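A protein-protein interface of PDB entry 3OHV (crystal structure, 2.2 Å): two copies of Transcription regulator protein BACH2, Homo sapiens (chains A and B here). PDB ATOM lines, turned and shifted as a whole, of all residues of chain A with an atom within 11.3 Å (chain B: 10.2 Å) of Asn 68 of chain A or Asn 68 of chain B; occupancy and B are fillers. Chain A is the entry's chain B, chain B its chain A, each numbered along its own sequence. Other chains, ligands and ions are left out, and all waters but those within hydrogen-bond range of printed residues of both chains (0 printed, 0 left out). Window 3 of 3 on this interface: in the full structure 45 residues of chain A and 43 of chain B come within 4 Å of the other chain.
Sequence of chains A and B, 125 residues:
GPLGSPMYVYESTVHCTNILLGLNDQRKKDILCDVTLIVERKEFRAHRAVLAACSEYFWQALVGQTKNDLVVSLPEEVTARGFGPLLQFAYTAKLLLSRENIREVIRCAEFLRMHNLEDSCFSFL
Leu 32 of chain A touches Arg 48 of chain B, and with the chains exchanged Arg 48 of chain A touches Leu 32 of chain B. Leu 32 of chain A touches Leu 62 of chain B, and with the chains exchanged Leu 62 of chain A touches Leu 32 of chain B. Lys 67 of chain A touches Asn 68 of chain B, but with the chains exchanged Asn 68 of chain A does not touch Lys 67 of chain B (7.1 Å). Asn 68 of chain A touches its own counterpart, Asn 68 of chain B. Positions printed for both chains: 32, 33, 34, 35, 36, 45, 46, 48, 62, 64, 65, 66, 67, 68, 69, 70, 71 and 72.
Printed residues of chain B within 4 Å of Leu 62 of chain A: Leu 32 (3.5 Å). No residue of chain B comes within 4 Å of Asp 69 of chain A. Of the printed residues of chain A, Leu 32 of chain B touches Arg 48, Leu 62 and Val 63. Of the printed residues of chain A, Arg 48 of chain B touches Leu 32. No residue of chain A comes within 4 Å of Thr 66 of chain B. No residue of chain A comes within 4 Å of Lys 67 of chain B. Of the printed residues of chain A, Asn 68 of chain B touches Lys 67 (3.0 Å) and Asn 68 (3.1 Å). No residue of chain A comes within 4 Å of Asp 69 of chain B. No residue of chain A comes within 4 Å of Leu 70 of chain B. The nearest residue of chain B that does not touch Asn 68 of chain A is Thr 66 of chain B (6.4 Å). The nearest printed residue of chain A that does not touch Arg 48 of chain B is Cys 33 of chain A (6.2 Å).
O of Leu 32 of chain B lies close to NE2 of His 47 of chain B (3.5 Å). The side-chain carboxylate of Asp 34 of chain B lies within salt-bridge range of the guanidinium group of Arg 48 of chain B (3.0 Å). The guanidinium group (NH2) of Arg 48 of chain B lies within hydrogen-bond range of the backbone carbonyl oxygen (O) of Lys 67 of chain B (2.7 Å). NH1 of Arg 48 of chain A sits at hydrogen-bond distance from O of Gln 65 of chain A (3.2 Å). The backbone carbonyl oxygen of Gln 65 of chain B lies within hydrogen-bond range of the guanidinium group of Arg 48 of chain B, 2.8 Å away. The side-chain carboxylate (OD2) of Asp 34 of chain A lies within salt-bridge range of the guanidinium group (NE) of Arg 48 of chain A (2.8 Å).
Printed residues of chain A that touch a printed residue of chain B: Leu 32, Arg 48, Leu 62, Val 63, Lys 67 and Asn 68. Hydrophobic or aromatic side chains of chain A that line the printed part of chain B: Leu 32 and Val 63. Along chain B the printed residues that touch a printed residue of chain A span positions 32 to 68. Among the printed residues, 7 pairs touch across the chains. Among the printed residues, no Asp or Glu carboxylate lies within 4 Å of a Lys or Arg side-chain nitrogen of the other chain.
The side-chain amide nitrogen (ND2) of Asn 68 of chain B lies within hydrogen-bond range of the backbone carbonyl oxygen (O) of Lys 67 of chain A, at 3.0 Å.
Arg 48 of chain B touches Leu 32 of chain A. CD2 of Leu 32 of chain A touches O of Leu 62 of chain B (3.4 Å). CD of Arg 48 of chain A touches CD2 of Leu 32 of chain B, 3.7 Å away. CD2 of Leu 32 of chain B touches O of Leu 62 of chain A, at 3.5 Å. Leu 32 of chain B touches Val 63 of chain A. Asn 68 of chain B touches Asn 68 of chain A (OD1 to CA, 3.1 Å).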
ATOM      1  N   LEU A  32     -20.930  14.484  -4.247  1.00  0.00           N
ATOM      2  CA  LEU A  32     -20.266  15.544  -5.016  1.00  0.00           C
ATOM      3  C   LEU A  32     -21.083  16.827  -5.251  1.00  0.00           C
ATOM      4  O   LEU A  32     -20.772  17.610  -6.161  1.00  0.00           O
ATOM      5  CB  LEU A  32     -19.750  15.001  -6.353  1.00  0.00           C
ATOM      6  CG  LEU A  32     -18.617  13.980  -6.298  1.00  0.00           C
ATOM      7  CD1 LEU A  32     -18.455  13.324  -7.640  1.00  0.00           C
ATOM      8  CD2 LEU A  32     -17.338  14.618  -5.887  1.00  0.00           C
ATOM      9  N   CYS A  33     -22.100  17.044  -4.426  1.00  0.00           N
ATOM     10  CA  CYS A  33     -22.880  18.258  -4.492  1.00  0.00           C
ATOM     11  C   CYS A  33     -22.122  19.378  -3.816  1.00  0.00           C
ATOM     12  O   CYS A  33     -21.036  19.161  -3.319  1.00  0.00           O
ATOM     13  CB  CYS A  33     -24.268  18.040  -3.880  1.00  0.00           C
ATOM     14  SG  CYS A  33     -25.296  17.003  -4.966  1.00  0.00           S
ATOM     15  N   ASP A  34     -22.671  20.588  -3.808  1.00  0.00           N
ATOM     16  CA  ASP A  34     -21.910  21.704  -3.247  1.00  0.00           C
ATOM     17  C   ASP A  34     -22.752  22.796  -2.618  1.00  0.00           C
ATOM     18  O   ASP A  34     -22.224  23.665  -1.950  1.00  0.00           O
ATOM     19  CB  ASP A  34     -20.954  22.298  -4.293  1.00  0.00           C
ATOM     20  CG  ASP A  34     -21.664  22.695  -5.588  1.00  0.00           C
ATOM     21  OD1 ASP A  34     -21.552  21.939  -6.587  1.00  0.00           O
ATOM     22  OD2 ASP A  34     -22.326  23.759  -5.606  1.00  0.00           O
ATOM     23  N   VAL A  35     -24.059  22.768  -2.824  1.00  0.00           N
ATOM     24  CA  VAL A  35     -24.902  23.812  -2.250  1.00  0.00           C
ATOM     25  C   VAL A  35     -26.120  23.157  -1.658  1.00  0.00           C
ATOM     26  O   VAL A  35     -26.604  22.152  -2.168  1.00  0.00           O
ATOM     27  CB  VAL A  35     -25.246  24.939  -3.293  1.00  0.00           C
ATOM     28  CG1 VAL A  35     -25.966  24.374  -4.497  1.00  0.00           C
ATOM     29  CG2 VAL A  35     -26.048  26.058  -2.681  1.00  0.00           C
ATOM     30  N   THR A  36     -26.568  23.683  -0.528  1.00  0.00           N
ATOM     31  CA  THR A  36     -27.823  23.271   0.060  1.00  0.00           C
ATOM     32  C   THR A  36     -28.763  24.453  -0.081  1.00  0.00           C
ATOM     33  O   THR A  36     -28.488  25.540   0.425  1.00  0.00           O
ATOM     34  CB  THR A  36     -27.692  22.817   1.545  1.00  0.00           C
ATOM     35  OG1 THR A  36     -26.861  21.647   1.629  1.00  0.00           O
ATOM     36  CG2 THR A  36     -29.082  22.451   2.109  1.00  0.00           C
ATOM     37  N   ARG A  45     -30.210  19.236  -1.979  1.00  0.00           N
ATOM     38  CA  ARG A  45     -28.835  19.286  -2.439  1.00  0.00           C
ATOM     39  C   ARG A  45     -28.788  19.433  -3.965  1.00  0.00           C
ATOM     40  O   ARG A  45     -29.639  18.900  -4.682  1.00  0.00           O
ATOM     41  CB  ARG A  45     -28.038  18.079  -1.948  1.00  0.00           C
ATOM     42  CG  ARG A  45     -27.920  17.974  -0.410  1.00  0.00           C
ATOM     43  CD  ARG A  45     -26.856  18.916   0.184  1.00  0.00           C
ATOM     44  NE  ARG A  45     -25.490  18.492  -0.125  1.00  0.00           N
ATOM     45  CZ  ARG A  45     -24.433  19.303  -0.117  1.00  0.00           C
ATOM     46  NH1 ARG A  45     -24.585  20.596   0.174  1.00  0.00           N
ATOM     47  NH2 ARG A  45     -23.220  18.819  -0.407  1.00  0.00           N
ATOM     48  N   ALA A  46     -27.825  20.210  -4.445  1.00  0.00           N
ATOM     49  CA  ALA A  46     -27.607  20.369  -5.871  1.00  0.00           C
ATOM     50  C   ALA A  46     -26.162  20.765  -6.147  1.00  0.00           C
ATOM     51  O   ALA A  46     -25.352  20.922  -5.221  1.00  0.00           O
ATOM     52  CB  ALA A  46     -28.558  21.413  -6.436  1.00  0.00           C
ATOM     53  N   ARG A  48     -24.252  23.828  -7.743  1.00  0.00           N
ATOM     54  CA  ARG A  48     -24.496  25.216  -8.128  1.00  0.00           C
ATOM     55  C   ARG A  48     -24.282  25.448  -9.623  1.00  0.00           C
ATOM     56  O   ARG A  48     -24.970  26.277 -10.226  1.00  0.00           O
ATOM     57  CB  ARG A  48     -23.647  26.177  -7.308  1.00  0.00           C
ATOM     58  CG  ARG A  48     -22.162  26.146  -7.648  1.00  0.00           C
ATOM     59  CD  ARG A  48     -21.347  26.976  -6.656  1.00  0.00           C
ATOM     60  NE  ARG A  48     -21.251  26.313  -5.359  1.00  0.00           N
ATOM     61  CZ  ARG A  48     -20.610  26.807  -4.299  1.00  0.00           C
ATOM     62  NH1 ARG A  48     -20.006  27.989  -4.361  1.00  0.00           N
ATOM     63  NH2 ARG A  48     -20.595  26.115  -3.167  1.00  0.00           N
ATOM     64  N   LEU A  62     -25.614  32.451  -6.919  1.00  0.00           N
ATOM     65  CA  LEU A  62     -24.566  31.495  -6.550  1.00  0.00           C
ATOM     66  C   LEU A  62     -23.113  31.749  -7.023  1.00  0.00           C
ATOM     67  O   LEU A  62     -22.218  31.010  -6.634  1.00  0.00           O
ATOM     68  CB  LEU A  62     -25.000  30.087  -6.978  1.00  0.00           C
ATOM     69  CG  LEU A  62     -26.383  29.582  -6.546  1.00  0.00           C
ATOM     70  CD1 LEU A  62     -26.833  28.439  -7.434  1.00  0.00           C
ATOM     71  CD2 LEU A  62     -26.422  29.189  -5.070  1.00  0.00           C
ATOM     72  N   VAL A  63     -22.885  32.775  -7.841  1.00  0.00           N
ATOM     73  CA  VAL A  63     -21.549  33.005  -8.422  1.00  0.00           C
ATOM     74  C   VAL A  63     -20.443  33.391  -7.437  1.00  0.00           C
ATOM     75  O   VAL A  63     -19.376  32.772  -7.439  1.00  0.00           O
ATOM     76  CB  VAL A  63     -21.575  34.014  -9.588  1.00  0.00           C
ATOM     77  CG1 VAL A  63     -20.172  34.518  -9.889  1.00  0.00           C
ATOM     78  CG2 VAL A  63     -22.147  33.363 -10.805  1.00  0.00           C
ATOM     79  N   GLY A  64     -20.678  34.405  -6.607  1.00  0.00           N
ATOM     80  CA  GLY A  64     -19.626  34.882  -5.693  1.00  0.00           C
ATOM     81  C   GLY A  64     -19.260  33.825  -4.671  1.00  0.00           C
ATOM     82  O   GLY A  64     -18.094  33.472  -4.509  1.00  0.00           O
ATOM     83  N   GLN A  65     -20.305  33.280  -4.053  1.00  0.00           N
ATOM     84  CA  GLN A  65     -20.259  32.405  -2.875  1.00  0.00           C
ATOM     85  C   GLN A  65     -18.996  31.561  -2.675  1.00  0.00           C
ATOM     86  O   GLN A  65     -18.637  30.719  -3.494  1.00  0.00           O
ATOM     87  CB  GLN A  65     -21.534  31.557  -2.840  1.00  0.00           C
ATOM     88  CG  GLN A  65     -22.811  32.319  -3.297  1.00  0.00           C
ATOM     89  CD  GLN A  65     -23.067  33.645  -2.555  1.00  0.00           C
ATOM     90  OE1 GLN A  65     -22.428  33.947  -1.556  1.00  0.00           O
ATOM     91  NE2 GLN A  65     -24.015  34.430  -3.052  1.00  0.00           N
ATOM     92  N   THR A  66     -18.310  31.834  -1.575  1.00  0.00           N
ATOM     93  CA  THR A  66     -17.032  31.204  -1.274  1.00  0.00           C
ATOM     94  C   THR A  66     -17.084  30.779   0.172  1.00  0.00           C
ATOM     95  O   THR A  66     -16.611  31.496   1.063  1.00  0.00           O
ATOM     96  CB  THR A  66     -15.831  32.169  -1.471  1.00  0.00           C
ATOM     97  OG1 THR A  66     -16.182  33.474  -0.995  1.00  0.00           O
ATOM     98  CG2 THR A  66     -15.418  32.262  -2.934  1.00  0.00           C
ATOM     99  N   LYS A  67     -17.668  29.607   0.404  1.00  0.00           N
ATOM    100  CA  LYS A  67     -17.873  29.072   1.744  1.00  0.00           C
ATOM    101  C   LYS A  67     -17.727  27.553   1.712  1.00  0.00           C
ATOM    102  O   LYS A  67     -18.005  26.917   0.690  1.00  0.00           O
ATOM    103  CB  LYS A  67     -19.284  29.432   2.235  1.00  0.00           C
ATOM    104  CG  LYS A  67     -19.475  29.393   3.752  1.00  0.00           C
ATOM    105  CD  LYS A  67     -20.898  28.973   4.143  1.00  0.00           C
ATOM    106  CE  LYS A  67     -21.961  29.757   3.386  1.00  0.00           C
ATOM    107  NZ  LYS A  67     -23.337  29.377   3.810  1.00  0.00           N
ATOM    108  N   ASN A  68     -17.273  26.980   2.824  1.00  0.00           N
ATOM    109  CA  ASN A  68     -17.395  25.556   3.045  1.00  0.00           C
ATOM    110  C   ASN A  68     -18.888  25.309   3.216  1.00  0.00           C
ATOM    111  O   ASN A  68     -19.593  26.138   3.800  1.00  0.00           O
ATOM    112  CB  ASN A  68     -16.633  25.147   4.304  1.00  0.00           C
ATOM    113  CG  ASN A  68     -17.119  25.883   5.546  1.00  0.00           C
ATOM    114  OD1 ASN A  68     -16.759  27.042   5.780  1.00  0.00           O
ATOM    115  ND2 ASN A  68     -17.947  25.213   6.347  1.00  0.00           N
ATOM    116  N   ASP A  69     -19.380  24.196   2.689  1.00  0.00           N
ATOM    117  CA  ASP A  69     -20.797  23.864   2.804  1.00  0.00           C
ATOM    118  C   ASP A  69     -21.720  25.099   2.654  1.00  0.00           C
ATOM    119  O   ASP A  69     -22.254  25.620   3.646  1.00  0.00           O
ATOM    120  CB  ASP A  69     -21.058  23.119   4.125  1.00  0.00           C
ATOM    121  CG  ASP A  69     -22.304  22.243   4.064  1.00  0.00           C
ATOM    122  OD1 ASP A  69     -22.233  21.109   3.526  1.00  0.00           O
ATOM    123  OD2 ASP A  69     -23.355  22.699   4.562  1.00  0.00           O
ATOM    124  N   LEU A  70     -21.886  25.564   1.414  1.00  0.00           N
ATOM    125  CA  LEU A  70     -22.758  26.710   1.112  1.00  0.00           C
ATOM    126  C   LEU A  70     -24.240  26.390   1.345  1.00  0.00           C
ATOM    127  O   LEU A  70     -24.698  25.288   1.030  1.00  0.00           O
ATOM    128  CB  LEU A  70     -22.541  27.181  -0.332  1.00  0.00           C
ATOM    129  CG  LEU A  70     -23.478  28.248  -0.913  1.00  0.00           C
ATOM    130  CD1 LEU A  70     -23.338  29.591  -0.210  1.00  0.00           C
ATOM    131  CD2 LEU A  70     -23.255  28.414  -2.403  1.00  0.00           C
ATOM    132  N   VAL A  71     -24.967  27.356   1.907  1.00  0.00           N
ATOM    133  CA  VAL A  71     -26.394  27.219   2.213  1.00  0.00           C
ATOM    134  C   VAL A  71     -27.159  28.474   1.795  1.00  0.00           C
ATOM    135  O   VAL A  71     -26.997  29.539   2.401  1.00  0.00           O
ATOM    136  CB  VAL A  71     -26.678  26.926   3.727  1.00  0.00           C
ATOM    137  CG1 VAL A  71     -28.179  27.023   4.021  1.00  0.00           C
ATOM    138  CG2 VAL A  71     -26.164  25.545   4.134  1.00  0.00           C
ATOM    139  N   VAL A  72     -28.004  28.332   0.776  1.00  0.00           N
ATOM    140  CA  VAL A  72     -28.806  29.442   0.258  1.00  0.00           C
ATOM    141  C   VAL A  72     -30.307  29.204   0.512  1.00  0.00           C
ATOM    142  O   VAL A  72     -30.857  28.152   0.180  1.00  0.00           O
ATOM    143  CB  VAL A  72     -28.501  29.707  -1.254  1.00  0.00           C
ATOM    144  CG1 VAL A  72     -29.421  30.777  -1.838  1.00  0.00           C
ATOM    145  CG2 VAL A  72     -27.037  30.110  -1.432  1.00  0.00           C
ATOM    146  N   LEU B  32     -17.641  29.519 -11.412  1.00  0.00           N
ATOM    147  CA  LEU B  32     -18.441  28.374 -10.885  1.00  0.00           C
ATOM    148  C   LEU B  32     -17.799  26.994 -11.026  1.00  0.00           C
ATOM    149  O   LEU B  32     -18.462  25.945 -10.784  1.00  0.00           O
ATOM    150  CB  LEU B  32     -19.898  28.349 -11.417  1.00  0.00           C
ATOM    151  CG  LEU B  32     -20.756  29.535 -10.935  1.00  0.00           C
ATOM    152  CD1 LEU B  32     -21.828  30.012 -11.946  1.00  0.00           C
ATOM    153  CD2 LEU B  32     -21.340  29.292  -9.560  1.00  0.00           C
ATOM    154  N   CYS B  33     -16.503  26.999 -11.362  1.00  0.00           N
ATOM    155  CA  CYS B  33     -15.692  25.790 -11.368  1.00  0.00           C
ATOM    156  C   CYS B  33     -15.255  25.451  -9.949  1.00  0.00           C
ATOM    157  O   CYS B  33     -15.444  26.238  -9.025  1.00  0.00           O
ATOM    158  CB  CYS B  33     -14.493  25.986 -12.297  1.00  0.00           C
ATOM    159  SG  CYS B  33     -14.973  25.862 -14.029  1.00  0.00           S
ATOM    160  N   ASP B  34     -14.666  24.279  -9.757  1.00  0.00           N
ATOM    161  CA  ASP B  34     -14.390  23.809  -8.398  1.00  0.00           C
ATOM    162  C   ASP B  34     -13.148  22.945  -8.258  1.00  0.00           C
ATOM    163  O   ASP B  34     -12.673  22.736  -7.146  1.00  0.00           O
ATOM    164  CB  ASP B  34     -15.608  23.075  -7.826  1.00  0.00           C
ATOM    165  CG  ASP B  34     -16.059  21.931  -8.694  1.00  0.00           C
ATOM    166  OD1 ASP B  34     -15.463  20.843  -8.614  1.00  0.00           O
ATOM    167  OD2 ASP B  34     -17.038  22.113  -9.461  1.00  0.00           O
ATOM    168  N   VAL B  35     -12.629  22.406  -9.356  1.00  0.00           N
ATOM    169  CA  VAL B  35     -11.358  21.684  -9.288  1.00  0.00           C
ATOM    170  C   VAL B  35     -10.320  22.232 -10.298  1.00  0.00           C
ATOM    171  O   VAL B  35     -10.688  22.679 -11.365  1.00  0.00           O
ATOM    172  CB  VAL B  35     -11.569  20.178  -9.461  1.00  0.00           C
ATOM    173  CG1 VAL B  35     -11.968  19.830 -10.892  1.00  0.00           C
ATOM    174  CG2 VAL B  35     -10.315  19.396  -9.042  1.00  0.00           C
ATOM    175  N   THR B  36      -9.039  22.217  -9.934  1.00  0.00           N
ATOM    176  CA  THR B  36      -7.954  22.515 -10.879  1.00  0.00           C
ATOM    177  C   THR B  36      -7.172  21.243 -11.173  1.00  0.00           C
ATOM    178  O   THR B  36      -6.615  20.628 -10.261  1.00  0.00           O
ATOM    179  CB  THR B  36      -6.971  23.582 -10.345  1.00  0.00           C
ATOM    180  OG1 THR B  36      -7.682  24.777 -10.018  1.00  0.00           O
ATOM    181  CG2 THR B  36      -5.883  23.913 -11.422  1.00  0.00           C
ATOM    182  N   ARG B  45      -9.037  24.183 -15.356  1.00  0.00           N
ATOM    183  CA  ARG B  45     -10.196  24.339 -14.472  1.00  0.00           C
ATOM    184  C   ARG B  45     -11.395  23.509 -14.949  1.00  0.00           C
ATOM    185  O   ARG B  45     -11.670  23.451 -16.144  1.00  0.00           O
ATOM    186  CB  ARG B  45     -10.577  25.829 -14.327  1.00  0.00           C
ATOM    187  CG  ARG B  45      -9.581  26.674 -13.502  1.00  0.00           C
ATOM    188  CD  ARG B  45      -9.585  26.268 -12.014  1.00  0.00           C
ATOM    189  NE  ARG B  45     -10.733  26.787 -11.272  1.00  0.00           N
ATOM    190  CZ  ARG B  45     -11.100  26.395 -10.051  1.00  0.00           C
ATOM    191  NH1 ARG B  45     -10.417  25.458  -9.369  1.00  0.00           N
ATOM    192  NH2 ARG B  45     -12.166  26.949  -9.501  1.00  0.00           N
ATOM    193  N   ALA B  46     -12.096  22.857 -14.032  1.00  0.00           N
ATOM    194  CA  ALA B  46     -13.293  22.066 -14.375  1.00  0.00           C
ATOM    195  C   ALA B  46     -14.245  21.955 -13.179  1.00  0.00           C
ATOM    196  O   ALA B  46     -14.094  22.693 -12.199  1.00  0.00           O
ATOM    197  CB  ALA B  46     -12.906  20.662 -14.898  1.00  0.00           C
ATOM    198  N   HIS B  47     -15.230  21.046 -13.290  1.00  0.00           N
ATOM    199  CA  HIS B  47     -16.161  20.742 -12.224  1.00  0.00           C
ATOM    200  C   HIS B  47     -15.972  19.273 -11.900  1.00  0.00           C
ATOM    201  O   HIS B  47     -16.104  18.428 -12.767  1.00  0.00           O
ATOM    202  CB  HIS B  47     -17.633  20.914 -12.644  1.00  0.00           C
ATOM    203  CG  HIS B  47     -17.960  22.213 -13.284  1.00  0.00           C
ATOM    204  ND1 HIS B  47     -17.744  22.454 -14.625  1.00  0.00           N
ATOM    205  CD2 HIS B  47     -18.549  23.328 -12.789  1.00  0.00           C
ATOM    206  CE1 HIS B  47     -18.150  23.678 -14.914  1.00  0.00           C
ATOM    207  NE2 HIS B  47     -18.637  24.232 -13.818  1.00  0.00           N
ATOM    208  N   ARG B  48     -15.680  18.966 -10.643  1.00  0.00           N
ATOM    209  CA  ARG B  48     -15.448  17.579 -10.233  1.00  0.00           C
ATOM    210  C   ARG B  48     -16.642  16.672 -10.500  1.00  0.00           C
ATOM    211  O   ARG B  48     -16.480  15.467 -10.800  1.00  0.00           O
ATOM    212  CB  ARG B  48     -15.056  17.510  -8.762  1.00  0.00           C
ATOM    213  CG  ARG B  48     -16.125  18.025  -7.828  1.00  0.00           C
ATOM    214  CD  ARG B  48     -15.622  18.091  -6.399  1.00  0.00           C
ATOM    215  NE  ARG B  48     -14.890  19.321  -6.148  1.00  0.00           N
ATOM    216  CZ  ARG B  48     -14.550  19.757  -4.943  1.00  0.00           C
ATOM    217  NH1 ARG B  48     -14.871  19.049  -3.853  1.00  0.00           N
ATOM    218  NH2 ARG B  48     -13.888  20.904  -4.841  1.00  0.00           N
ATOM    219  N   LEU B  62     -12.322  11.228  -7.192  1.00  0.00           N
ATOM    220  CA  LEU B  62     -12.979  12.437  -6.706  1.00  0.00           C
ATOM    221  C   LEU B  62     -14.137  12.255  -5.741  1.00  0.00           C
ATOM    222  O   LEU B  62     -14.428  13.157  -4.959  1.00  0.00           O
ATOM    223  CB  LEU B  62     -13.385  13.374  -7.848  1.00  0.00           C
ATOM    224  CG  LEU B  62     -12.301  13.905  -8.797  1.00  0.00           C
ATOM    225  CD1 LEU B  62     -12.988  14.539  -9.985  1.00  0.00           C
ATOM    226  CD2 LEU B  62     -11.355  14.916  -8.131  1.00  0.00           C
ATOM    227  N   GLY B  64     -16.031  11.692  -2.532  1.00  0.00           N
ATOM    228  CA  GLY B  64     -15.577  11.897  -1.148  1.00  0.00           C
ATOM    229  C   GLY B  64     -14.677  13.109  -0.932  1.00  0.00           C
ATOM    230  O   GLY B  64     -14.321  13.416   0.213  1.00  0.00           O
ATOM    231  N   GLN B  65     -14.276  13.779  -2.019  1.00  0.00           N
ATOM    232  CA  GLN B  65     -13.549  15.040  -1.904  1.00  0.00           C
ATOM    233  C   GLN B  65     -14.591  16.130  -1.700  1.00  0.00           C
ATOM    234  O   GLN B  65     -15.293  16.520  -2.639  1.00  0.00           O
ATOM    235  CB  GLN B  65     -12.680  15.366  -3.140  1.00  0.00           C
ATOM    236  CG  GLN B  65     -11.739  14.263  -3.646  1.00  0.00           C
ATOM    237  CD  GLN B  65     -10.603  13.919  -2.686  1.00  0.00           C
ATOM    238  OE1 GLN B  65     -10.482  14.498  -1.605  1.00  0.00           O
ATOM    239  NE2 GLN B  65      -9.764  12.967  -3.087  1.00  0.00           N
ATOM    240  N   THR B  66     -14.672  16.612  -0.466  1.00  0.00           N
ATOM    241  CA  THR B  66     -15.685  17.556  -0.023  1.00  0.00           C
ATOM    242  C   THR B  66     -15.140  18.988   0.065  1.00  0.00           C
ATOM    243  O   THR B  66     -15.884  19.960   0.259  1.00  0.00           O
ATOM    244  CB  THR B  66     -16.170  17.144   1.376  1.00  0.00           C
ATOM    245  OG1 THR B  66     -17.174  18.061   1.816  1.00  0.00           O
ATOM    246  CG2 THR B  66     -14.997  17.141   2.380  1.00  0.00           C
ATOM    247  N   LYS B  67     -13.825  19.091  -0.051  1.00  0.00           N
ATOM    248  CA  LYS B  67     -13.093  20.318   0.160  1.00  0.00           C
ATOM    249  C   LYS B  67     -13.341  21.305  -0.984  1.00  0.00           C
ATOM    250  O   LYS B  67     -13.544  20.905  -2.129  1.00  0.00           O
ATOM    251  CB  LYS B  67     -11.610  19.959   0.272  1.00  0.00           C
ATOM    252  CG  LYS B  67     -10.684  21.084   0.662  1.00  0.00           C
ATOM    253  CD  LYS B  67      -9.231  20.641   0.517  1.00  0.00           C
ATOM    254  CE  LYS B  67      -8.307  21.814   0.712  1.00  0.00           C
ATOM    255  NZ  LYS B  67      -7.040  21.347   1.327  1.00  0.00           N
ATOM    256  N   ASN B  68     -13.315  22.593  -0.660  1.00  0.00           N
ATOM    257  CA  ASN B  68     -13.542  23.659  -1.646  1.00  0.00           C
ATOM    258  C   ASN B  68     -12.407  23.874  -2.656  1.00  0.00           C
ATOM    259  O   ASN B  68     -12.599  23.716  -3.867  1.00  0.00           O
ATOM    260  CB  ASN B  68     -13.835  24.972  -0.921  1.00  0.00           C
ATOM    261  CG  ASN B  68     -15.171  24.959  -0.218  1.00  0.00           C
ATOM    262  OD1 ASN B  68     -15.230  24.716   1.011  1.00  0.00           O
ATOM    263  ND2 ASN B  68     -16.242  25.202  -0.954  1.00  0.00           N
ATOM    264  N   ASP B  69     -11.237  24.276  -2.167  1.00  0.00           N
ATOM    265  CA  ASP B  69     -10.073  24.448  -3.031  1.00  0.00           C
ATOM    266  C   ASP B  69      -9.550  23.046  -3.318  1.00  0.00           C
ATOM    267  O   ASP B  69      -9.063  22.371  -2.410  1.00  0.00           O
ATOM    268  CB  ASP B  69      -8.955  25.263  -2.339  1.00  0.00           C
ATOM    269  CG  ASP B  69      -9.399  26.668  -1.873  1.00  0.00           C
ATOM    270  OD1 ASP B  69     -10.469  27.188  -2.286  1.00  0.00           O
ATOM    271  OD2 ASP B  69      -8.624  27.263  -1.090  1.00  0.00           O
ATOM    272  N   LEU B  70      -9.666  22.589  -4.554  1.00  0.00           N
ATOM    273  CA  LEU B  70      -9.201  21.240  -4.881  1.00  0.00           C
ATOM    274  C   LEU B  70      -8.258  21.245  -6.083  1.00  0.00           C
ATOM    275  O   LEU B  70      -8.611  21.720  -7.159  1.00  0.00           O
ATOM    276  CB  LEU B  70     -10.378  20.275  -5.096  1.00  0.00           C
ATOM    277  CG  LEU B  70     -10.070  18.781  -5.299  1.00  0.00           C
ATOM    278  CD1 LEU B  70      -9.554  18.079  -4.033  1.00  0.00           C
ATOM    279  CD2 LEU B  70     -11.298  18.035  -5.809  1.00  0.00           C
ATOM    280  N   VAL B  71      -7.045  20.750  -5.878  1.00  0.00           N
ATOM    281  CA  VAL B  71      -6.098  20.601  -6.973  1.00  0.00           C
ATOM    282  C   VAL B  71      -5.769  19.120  -7.123  1.00  0.00           C
ATOM    283  O   VAL B  71      -5.506  18.436  -6.135  1.00  0.00           O
ATOM    284  CB  VAL B  71      -4.820  21.499  -6.823  1.00  0.00           C
ATOM    285  CG1 VAL B  71      -4.137  21.304  -5.483  1.00  0.00           C
ATOM    286  CG2 VAL B  71      -3.838  21.212  -7.910  1.00  0.00           C
ATOM    287  N   VAL B  72      -5.837  18.623  -8.356  1.00  0.00           N
ATOM    288  CA  VAL B  72      -5.645  17.204  -8.605  1.00  0.00           C
ATOM    289  C   VAL B  72      -4.549  17.030  -9.627  1.00  0.00           C
ATOM    290  O   VAL B  72      -4.675  17.489 -10.769  1.00  0.00           O
ATOM    291  CB  VAL B  72      -6.964  16.528  -9.106  1.00  0.00           C
ATOM    292  CG1 VAL B  72      -6.694  15.115  -9.636  1.00  0.00           C
ATOM    293  CG2 VAL B  72      -7.970  16.510  -8.007  1.00  0.00           C
